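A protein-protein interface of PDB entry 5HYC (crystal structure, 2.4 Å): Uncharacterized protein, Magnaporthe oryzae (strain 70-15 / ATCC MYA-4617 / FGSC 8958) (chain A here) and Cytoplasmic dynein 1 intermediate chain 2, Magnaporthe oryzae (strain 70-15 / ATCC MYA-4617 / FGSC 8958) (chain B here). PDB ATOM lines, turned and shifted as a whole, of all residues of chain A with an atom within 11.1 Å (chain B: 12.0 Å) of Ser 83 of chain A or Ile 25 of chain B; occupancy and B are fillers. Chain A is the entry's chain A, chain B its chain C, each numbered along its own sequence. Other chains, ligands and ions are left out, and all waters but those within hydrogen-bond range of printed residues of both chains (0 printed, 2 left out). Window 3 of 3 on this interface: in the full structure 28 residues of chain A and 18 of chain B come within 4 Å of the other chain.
A ring nitrogen (NE2) of His 108 of chain A lies within hydrogen-bond range of the backbone carbonyl oxygen of Pro 21 of chain B. The backbone carbonyl oxygen (O) of Lys 106 of chain A lies close to the side-chain amino group (NZ) of Lys 23 of chain B (3.1 Å). NZ of Lys 23 of chain B is in salt-bridge range of OE1 of Glu 138 of chain A, at 3.1 Å. The backbone NH (N) of Ser 82 of chain A lies within hydrogen-bond range of the side-chain carboxylate (OE2) of Glu 24 of chain B (2.9 Å). O of Asp 104 of chain A lies within hydrogen-bond range of NZ of Lys 23 of chain B, 3.1 Å away.
The backbone carbonyl oxygen (O) of Gly 110 of chain A is in hydrogen-bond range of the backbone NH (N) of Leu 79 of chain A (2.9 Å). The backbone NH of His 108 of chain A is in hydrogen-bond range of the side-chain carboxylate of Glu 138 of chain A, at 3.0 Å.
Leu 79 of chain A touches Val 22 of chain B. Val 80 of chain A touches Val 22 of chain B. N of Pro 81 of chain A touches CG2 of Val 22 of chain B, at 3.5 Å. Pro 81 of chain A touches Lys 23 of chain B (CB to O, 3.5 Å). C of Pro 81 of chain A touches OE2 of Glu 24 of chain B (3.8 Å). Pro 81 of chain A touches Ile 25 of chain B (CG to CD1, 3.8 Å). Ile 25 of chain B touches Ser 83 of chain A (CB to OG, 3.4 Å). His 108 of chain A touches Lys 23 of chain B (N to CE, 3.9 Å). Gly 110 of chain A touches Pro 21 of chain B. Val 22 of chain B touches Gly 110 of chain A.
Of the printed residues of chain B, Ser 83 of chain A touches Ile 25 (3.4 Å). Ile 25 of chain B touches just these residues of chain A: Pro 81 and Ser 83. Lys 84 of chain A touches none of the printed residues of chain B. Asp 104 of chain A touches just one residue of chain B: Lys 23. Lys 23 of chain B touches seven residues of chain A. Glu 24 of chain B touches two residues of chain A. No residue of chain A comes within 4 Å of Phe 26 of chain B. No residue of chain A comes within 4 Å of Ser 27 of chain B. Printed residues of chain A within 4 Å of Val 22 of chain B: Leu 79 (3.5 Å), Val 80 (3.6 Å), Pro 81 (3.5 Å) and Gly 110 (3.8 Å). Of the printed residues of chain B, Gly 110 of chain A touches Pro 21 and Val 22. Printed residues of chain B within 4 Å of Glu 138 of chain A: Lys 23. The nearest residue of chain A that does not touch Ile 25 of chain B is Lys 84 of chain A (4.7 Å).
Of the 14 printed residues of chain A, 12 touch a printed residue of chain B. Among the printed residues, 17 pairs touch across the chains. Among the printed residues, Asp or Glu carboxylates within 4 Å of a Lys or Arg side-chain nitrogen of the other chain: Glu 138 of chain A with Lys 23 of chain B (3.1 Å).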
ATOM      1  N   LEU A  79      -6.508 -21.434  -7.878  1.00  0.00           N
ATOM      2  CA  LEU A  79      -6.710 -20.001  -7.709  1.00  0.00           C
ATOM      3  C   LEU A  79      -7.388 -19.736  -6.375  1.00  0.00           C
ATOM      4  O   LEU A  79      -8.220 -20.499  -5.935  1.00  0.00           O
ATOM      5  CB  LEU A  79      -7.515 -19.421  -8.862  1.00  0.00           C
ATOM      6  CG  LEU A  79      -6.871 -19.526 -10.242  1.00  0.00           C
ATOM      7  CD1 LEU A  79      -7.732 -18.858 -11.307  1.00  0.00           C
ATOM      8  CD2 LEU A  79      -5.489 -18.923 -10.232  1.00  0.00           C
ATOM      9  N   VAL A  80      -6.955 -18.677  -5.719  1.00  0.00           N
ATOM     10  CA  VAL A  80      -7.418 -18.281  -4.398  1.00  0.00           C
ATOM     11  C   VAL A  80      -8.343 -17.075  -4.562  1.00  0.00           C
ATOM     12  O   VAL A  80      -7.999 -16.119  -5.254  1.00  0.00           O
ATOM     13  CB  VAL A  80      -6.219 -17.925  -3.468  1.00  0.00           C
ATOM     14  CG1 VAL A  80      -6.681 -17.596  -2.066  1.00  0.00           C
ATOM     15  CG2 VAL A  80      -5.170 -19.052  -3.476  1.00  0.00           C
ATOM     16  N   PRO A  81      -9.542 -17.136  -3.982  1.00  0.00           N
ATOM     17  CA  PRO A  81     -10.438 -15.983  -4.136  1.00  0.00           C
ATOM     18  C   PRO A  81      -9.860 -14.721  -3.537  1.00  0.00           C
ATOM     19  O   PRO A  81      -9.058 -14.782  -2.605  1.00  0.00           O
ATOM     20  CB  PRO A  81     -11.708 -16.414  -3.390  1.00  0.00           C
ATOM     21  CG  PRO A  81     -11.299 -17.582  -2.561  1.00  0.00           C
ATOM     22  CD  PRO A  81     -10.198 -18.262  -3.302  1.00  0.00           C
ATOM     23  N   SER A  82     -10.275 -13.594  -4.091  1.00  0.00           N
ATOM     24  CA  SER A  82      -9.856 -12.268  -3.644  1.00  0.00           C
ATOM     25  C   SER A  82      -9.991 -12.078  -2.136  1.00  0.00           C
ATOM     26  O   SER A  82      -9.119 -11.496  -1.501  1.00  0.00           O
ATOM     27  CB  SER A  82     -10.658 -11.203  -4.388  1.00  0.00           C
ATOM     28  OG  SER A  82     -10.159  -9.912  -4.118  1.00  0.00           O
ATOM     29  N   SER A  83     -11.070 -12.591  -1.562  1.00  0.00           N
ATOM     30  CA  SER A  83     -11.262 -12.531  -0.124  1.00  0.00           C
ATOM     31  C   SER A  83     -10.385 -13.516   0.672  1.00  0.00           C
ATOM     32  O   SER A  83     -10.413 -13.501   1.902  1.00  0.00           O
ATOM     33  CB  SER A  83     -12.734 -12.784   0.208  1.00  0.00           C
ATOM     34  OG  SER A  83     -13.075 -14.156   0.079  1.00  0.00           O
ATOM     35  N   LYS A  84      -9.616 -14.358  -0.024  1.00  0.00           N
ATOM     36  CA  LYS A  84      -8.788 -15.413   0.600  1.00  0.00           C
ATOM     37  C   LYS A  84      -9.632 -16.377   1.439  1.00  0.00           C
ATOM     38  O   LYS A  84      -9.992 -17.468   0.993  1.00  0.00           O
ATOM     39  CB  LYS A  84      -7.676 -14.813   1.479  1.00  0.00           C
ATOM     40  CG  LYS A  84      -6.371 -14.527   0.773  1.00  0.00           C
ATOM     41  CD  LYS A  84      -6.548 -13.488  -0.305  1.00  0.00           C
ATOM     42  CE  LYS A  84      -5.259 -13.268  -1.081  1.00  0.00           C
ATOM     43  NZ  LYS A  84      -5.518 -12.528  -2.343  1.00  0.00           N
ATOM     44  N   ASP A 104     -22.249 -19.911  -0.786  1.00  0.00           N
ATOM     45  CA  ASP A 104     -21.236 -20.768  -1.395  1.00  0.00           C
ATOM     46  C   ASP A 104     -21.557 -21.076  -2.848  1.00  0.00           C
ATOM     47  O   ASP A 104     -20.722 -20.896  -3.735  1.00  0.00           O
ATOM     48  CB  ASP A 104     -21.097 -22.082  -0.619  1.00  0.00           C
ATOM     49  CG  ASP A 104     -19.832 -22.140   0.212  1.00  0.00           C
ATOM     50  OD1 ASP A 104     -19.281 -21.069   0.534  1.00  0.00           O
ATOM     51  OD2 ASP A 104     -19.390 -23.256   0.548  1.00  0.00           O
ATOM     52  N   GLY A 105     -22.777 -21.546  -3.084  1.00  0.00           N
ATOM     53  CA  GLY A 105     -23.159 -22.054  -4.391  1.00  0.00           C
ATOM     54  C   GLY A 105     -22.466 -23.381  -4.662  1.00  0.00           C
ATOM     55  O   GLY A 105     -21.856 -23.955  -3.760  1.00  0.00           O
ATOM     56  N   LYS A 106     -22.548 -23.874  -5.896  1.00  0.00           N
ATOM     57  CA  LYS A 106     -21.855 -25.110  -6.248  1.00  0.00           C
ATOM     58  C   LYS A 106     -20.351 -24.975  -6.231  1.00  0.00           C
ATOM     59  O   LYS A 106     -19.803 -23.968  -6.678  1.00  0.00           O
ATOM     60  CB  LYS A 106     -22.274 -25.610  -7.624  1.00  0.00           C
ATOM     61  CG  LYS A 106     -23.754 -25.666  -7.791  1.00  0.00           C
ATOM     62  CD  LYS A 106     -24.275 -27.092  -7.520  1.00  0.00           C
ATOM     63  CE  LYS A 106     -25.520 -27.020  -6.593  1.00  0.00           C
ATOM     64  NZ  LYS A 106     -26.490 -26.072  -7.151  1.00  0.00           N
ATOM     65  N   PRO A 107     -19.679 -26.014  -5.732  1.00  0.00           N
ATOM     66  CA  PRO A 107     -18.222 -26.010  -5.734  1.00  0.00           C
ATOM     67  C   PRO A 107     -17.665 -25.829  -7.137  1.00  0.00           C
ATOM     68  O   PRO A 107     -18.215 -26.344  -8.113  1.00  0.00           O
ATOM     69  CB  PRO A 107     -17.857 -27.376  -5.145  1.00  0.00           C
ATOM     70  CG  PRO A 107     -19.102 -28.182  -5.182  1.00  0.00           C
ATOM     71  CD  PRO A 107     -20.230 -27.215  -5.088  1.00  0.00           C
ATOM     72  N   HIS A 108     -16.601 -25.044  -7.219  1.00  0.00           N
ATOM     73  CA  HIS A 108     -15.959 -24.721  -8.479  1.00  0.00           C
ATOM     74  C   HIS A 108     -14.486 -24.417  -8.240  1.00  0.00           C
ATOM     75  O   HIS A 108     -14.131 -23.671  -7.326  1.00  0.00           O
ATOM     76  CB  HIS A 108     -16.629 -23.528  -9.163  1.00  0.00           C
ATOM     77  CG  HIS A 108     -15.869 -23.018 -10.345  1.00  0.00           C
ATOM     78  ND1 HIS A 108     -15.918 -23.622 -11.581  1.00  0.00           N
ATOM     79  CD2 HIS A 108     -15.003 -21.980 -10.471  1.00  0.00           C
ATOM     80  CE1 HIS A 108     -15.133 -22.971 -12.423  1.00  0.00           C
ATOM     81  NE2 HIS A 108     -14.566 -21.972 -11.770  1.00  0.00           N
ATOM     82  N   GLY A 110     -11.095 -22.690  -9.496  1.00  0.00           N
ATOM     83  CA  GLY A 110     -10.371 -21.807 -10.388  1.00  0.00           C
ATOM     84  C   GLY A 110      -8.968 -22.350 -10.646  1.00  0.00           C
ATOM     85  O   GLY A 110      -8.270 -22.740  -9.730  1.00  0.00           O
ATOM     86  N   GLU A 138     -12.302 -28.513  -4.528  1.00  0.00           N
ATOM     87  CA  GLU A 138     -12.173 -27.117  -4.121  1.00  0.00           C
ATOM     88  C   GLU A 138     -11.542 -26.978  -2.737  1.00  0.00           C
ATOM     89  O   GLU A 138     -10.754 -26.071  -2.518  1.00  0.00           O
ATOM     90  CB  GLU A 138     -13.543 -26.413  -4.160  1.00  0.00           C
ATOM     91  CG  GLU A 138     -13.490 -24.906  -3.900  1.00  0.00           C
ATOM     92  CD  GLU A 138     -14.855 -24.273  -3.607  1.00  0.00           C
ATOM     93  OE1 GLU A 138     -15.814 -24.504  -4.371  1.00  0.00           O
ATOM     94  OE2 GLU A 138     -14.962 -23.528  -2.612  1.00  0.00           O
ATOM     95  N   SER A 139     -11.878 -27.881  -1.817  1.00  0.00           N
ATOM     96  CA  SER A 139     -11.370 -27.805  -0.456  1.00  0.00           C
ATOM     97  C   SER A 139      -9.884 -28.144  -0.361  1.00  0.00           C
ATOM     98  O   SER A 139      -9.200 -27.681   0.548  1.00  0.00           O
ATOM     99  CB  SER A 139     -12.148 -28.745   0.467  1.00  0.00           C
ATOM    100  OG  SER A 139     -11.748 -30.090   0.268  1.00  0.00           O
ATOM    101  N   PRO B  21     -12.155 -19.433 -14.085  1.00  0.00           N
ATOM    102  CA  PRO B  21     -12.179 -18.358 -13.098  1.00  0.00           C
ATOM    103  C   PRO B  21     -12.354 -18.893 -11.685  1.00  0.00           C
ATOM    104  O   PRO B  21     -13.000 -19.916 -11.488  1.00  0.00           O
ATOM    105  CB  PRO B  21     -13.375 -17.506 -13.547  1.00  0.00           C
ATOM    106  CG  PRO B  21     -14.261 -18.466 -14.250  1.00  0.00           C
ATOM    107  CD  PRO B  21     -13.361 -19.440 -14.934  1.00  0.00           C
ATOM    108  N   VAL B  22     -11.743 -18.203 -10.729  1.00  0.00           N
ATOM    109  CA  VAL B  22     -11.901 -18.498  -9.312  1.00  0.00           C
ATOM    110  C   VAL B  22     -13.337 -18.228  -8.855  1.00  0.00           C
ATOM    111  O   VAL B  22     -14.015 -17.370  -9.398  1.00  0.00           O
ATOM    112  CB  VAL B  22     -10.881 -17.672  -8.481  1.00  0.00           C
ATOM    113  CG1 VAL B  22     -11.304 -16.239  -8.360  1.00  0.00           C
ATOM    114  CG2 VAL B  22     -10.658 -18.286  -7.107  1.00  0.00           C
ATOM    115  N   LYS B  23     -13.821 -18.992  -7.881  1.00  0.00           N
ATOM    116  CA  LYS B  23     -15.113 -18.694  -7.280  1.00  0.00           C
ATOM    117  C   LYS B  23     -14.932 -17.625  -6.214  1.00  0.00           C
ATOM    118  O   LYS B  23     -14.403 -17.896  -5.154  1.00  0.00           O
ATOM    119  CB  LYS B  23     -15.746 -19.945  -6.668  1.00  0.00           C
ATOM    120  CG  LYS B  23     -17.070 -19.687  -5.960  1.00  0.00           C
ATOM    121  CD  LYS B  23     -17.312 -20.673  -4.819  1.00  0.00           C
ATOM    122  CE  LYS B  23     -18.027 -21.913  -5.306  1.00  0.00           C
ATOM    123  NZ  LYS B  23     -18.383 -22.843  -4.196  1.00  0.00           N
ATOM    124  N   GLU B  24     -15.368 -16.408  -6.496  1.00  0.00           N
ATOM    125  CA  GLU B  24     -15.211 -15.333  -5.536  1.00  0.00           C
ATOM    126  C   GLU B  24     -16.193 -15.471  -4.384  1.00  0.00           C
ATOM    127  O   GLU B  24     -17.285 -16.002  -4.538  1.00  0.00           O
ATOM    128  CB  GLU B  24     -15.376 -13.986  -6.222  1.00  0.00           C
ATOM    129  CG  GLU B  24     -14.324 -13.714  -7.272  1.00  0.00           C
ATOM    130  CD  GLU B  24     -12.965 -13.316  -6.697  1.00  0.00           C
ATOM    131  OE1 GLU B  24     -12.069 -12.983  -7.493  1.00  0.00           O
ATOM    132  OE2 GLU B  24     -12.792 -13.323  -5.465  1.00  0.00           O
ATOM    133  N   ILE B  25     -15.776 -14.996  -3.223  1.00  0.00           N
ATOM    134  CA  ILE B  25     -16.601 -15.038  -2.041  1.00  0.00           C
ATOM    135  C   ILE B  25     -17.011 -13.617  -1.664  1.00  0.00           C
ATOM    136  O   ILE B  25     -16.173 -12.745  -1.451  1.00  0.00           O
ATOM    137  CB  ILE B  25     -15.884 -15.718  -0.884  1.00  0.00           C
ATOM    138  CG1 ILE B  25     -15.556 -17.158  -1.274  1.00  0.00           C
ATOM    139  CG2 ILE B  25     -16.764 -15.709   0.355  1.00  0.00           C
ATOM    140  CD1 ILE B  25     -14.433 -17.768  -0.488  1.00  0.00           C
ATOM    141  N   PHE B  26     -18.316 -13.401  -1.593  1.00  0.00           N
ATOM    142  CA  PHE B  26     -18.846 -12.059  -1.483  1.00  0.00           C
ATOM    143  C   PHE B  26     -19.213 -11.718  -0.048  1.00  0.00           C
ATOM    144  O   PHE B  26     -19.304 -12.587   0.811  1.00  0.00           O
ATOM    145  CB  PHE B  26     -20.053 -11.897  -2.410  1.00  0.00           C
ATOM    146  CG  PHE B  26     -19.800 -12.360  -3.824  1.00  0.00           C
ATOM    147  CD1 PHE B  26     -18.816 -11.769  -4.598  1.00  0.00           C
ATOM    148  CD2 PHE B  26     -20.567 -13.378  -4.387  1.00  0.00           C
ATOM    149  CE1 PHE B  26     -18.588 -12.191  -5.903  1.00  0.00           C
ATOM    150  CE2 PHE B  26     -20.342 -13.799  -5.686  1.00  0.00           C
ATOM    151  CZ  PHE B  26     -19.344 -13.203  -6.441  1.00  0.00           C
ATOM    152  N   SER B  27     -19.396 -10.435   0.201  1.00  0.00           N
ATOM    153  CA  SER B  27     -19.800  -9.958   1.508  1.00  0.00           C
ATOM    154  C   SER B  27     -21.288  -9.600   1.488  1.00  0.00           C
ATOM    155  O   SER B  27     -21.763  -8.956   0.573  1.00  0.00           O
ATOM    156  CB  SER B  27     -18.965  -8.753   1.902  1.00  0.00           C
ATOM    157  OG  SER B  27     -17.596  -9.035   1.743  1.00  0.00           O
ATOM    158  N   TYR B  28     -22.005 -10.009   2.519  1.00  0.00           N
ATOM    159  CA  TYR B  28     -23.437  -9.856   2.562  1.00  0.00           C
ATOM    160  C   TYR B  28     -23.842  -8.968   3.728  1.00  0.00           C
ATOM    161  O   TYR B  28     -23.169  -8.919   4.743  1.00  0.00           O
ATOM    162  CB  TYR B  28     -24.100 -11.219   2.656  1.00  0.00           C
ATOM    163  CG  TYR B  28     -23.796 -12.082   1.456  1.00  0.00           C
ATOM    164  CD1 TYR B  28     -22.658 -12.878   1.420  1.00  0.00           C
ATOM    165  CD2 TYR B  28     -24.626 -12.080   0.344  1.00  0.00           C
ATOM    166  CE1 TYR B  28     -22.369 -13.654   0.330  1.00  0.00           C
ATOM    167  CE2 TYR B  28     -24.337 -12.851  -0.760  1.00  0.00           C
ATOM    168  CZ  TYR B  28     -23.209 -13.643  -0.756  1.00  0.00           C
ATOM    169  OH  TYR B  28     -22.915 -14.424  -1.843  1.00  0.00           O
ATOM    170  N   SER B  29     -24.928  -8.233   3.546  1.00  0.00           N
ATOM    171  CA  SER B  29     -25.524  -7.480   4.619  1.00  0.00           C
ATOM    172  C   SER B  29     -26.364  -8.393   5.487  1.00  0.00           C
ATOM    173  O   SER B  29     -26.510  -9.576   5.209  1.00  0.00           O
ATOM    174  CB  SER B  29     -26.382  -6.349   4.068  1.00  0.00           C
ATOM    175  OG  SER B  29     -27.477  -6.866   3.353  1.00  0.00           O
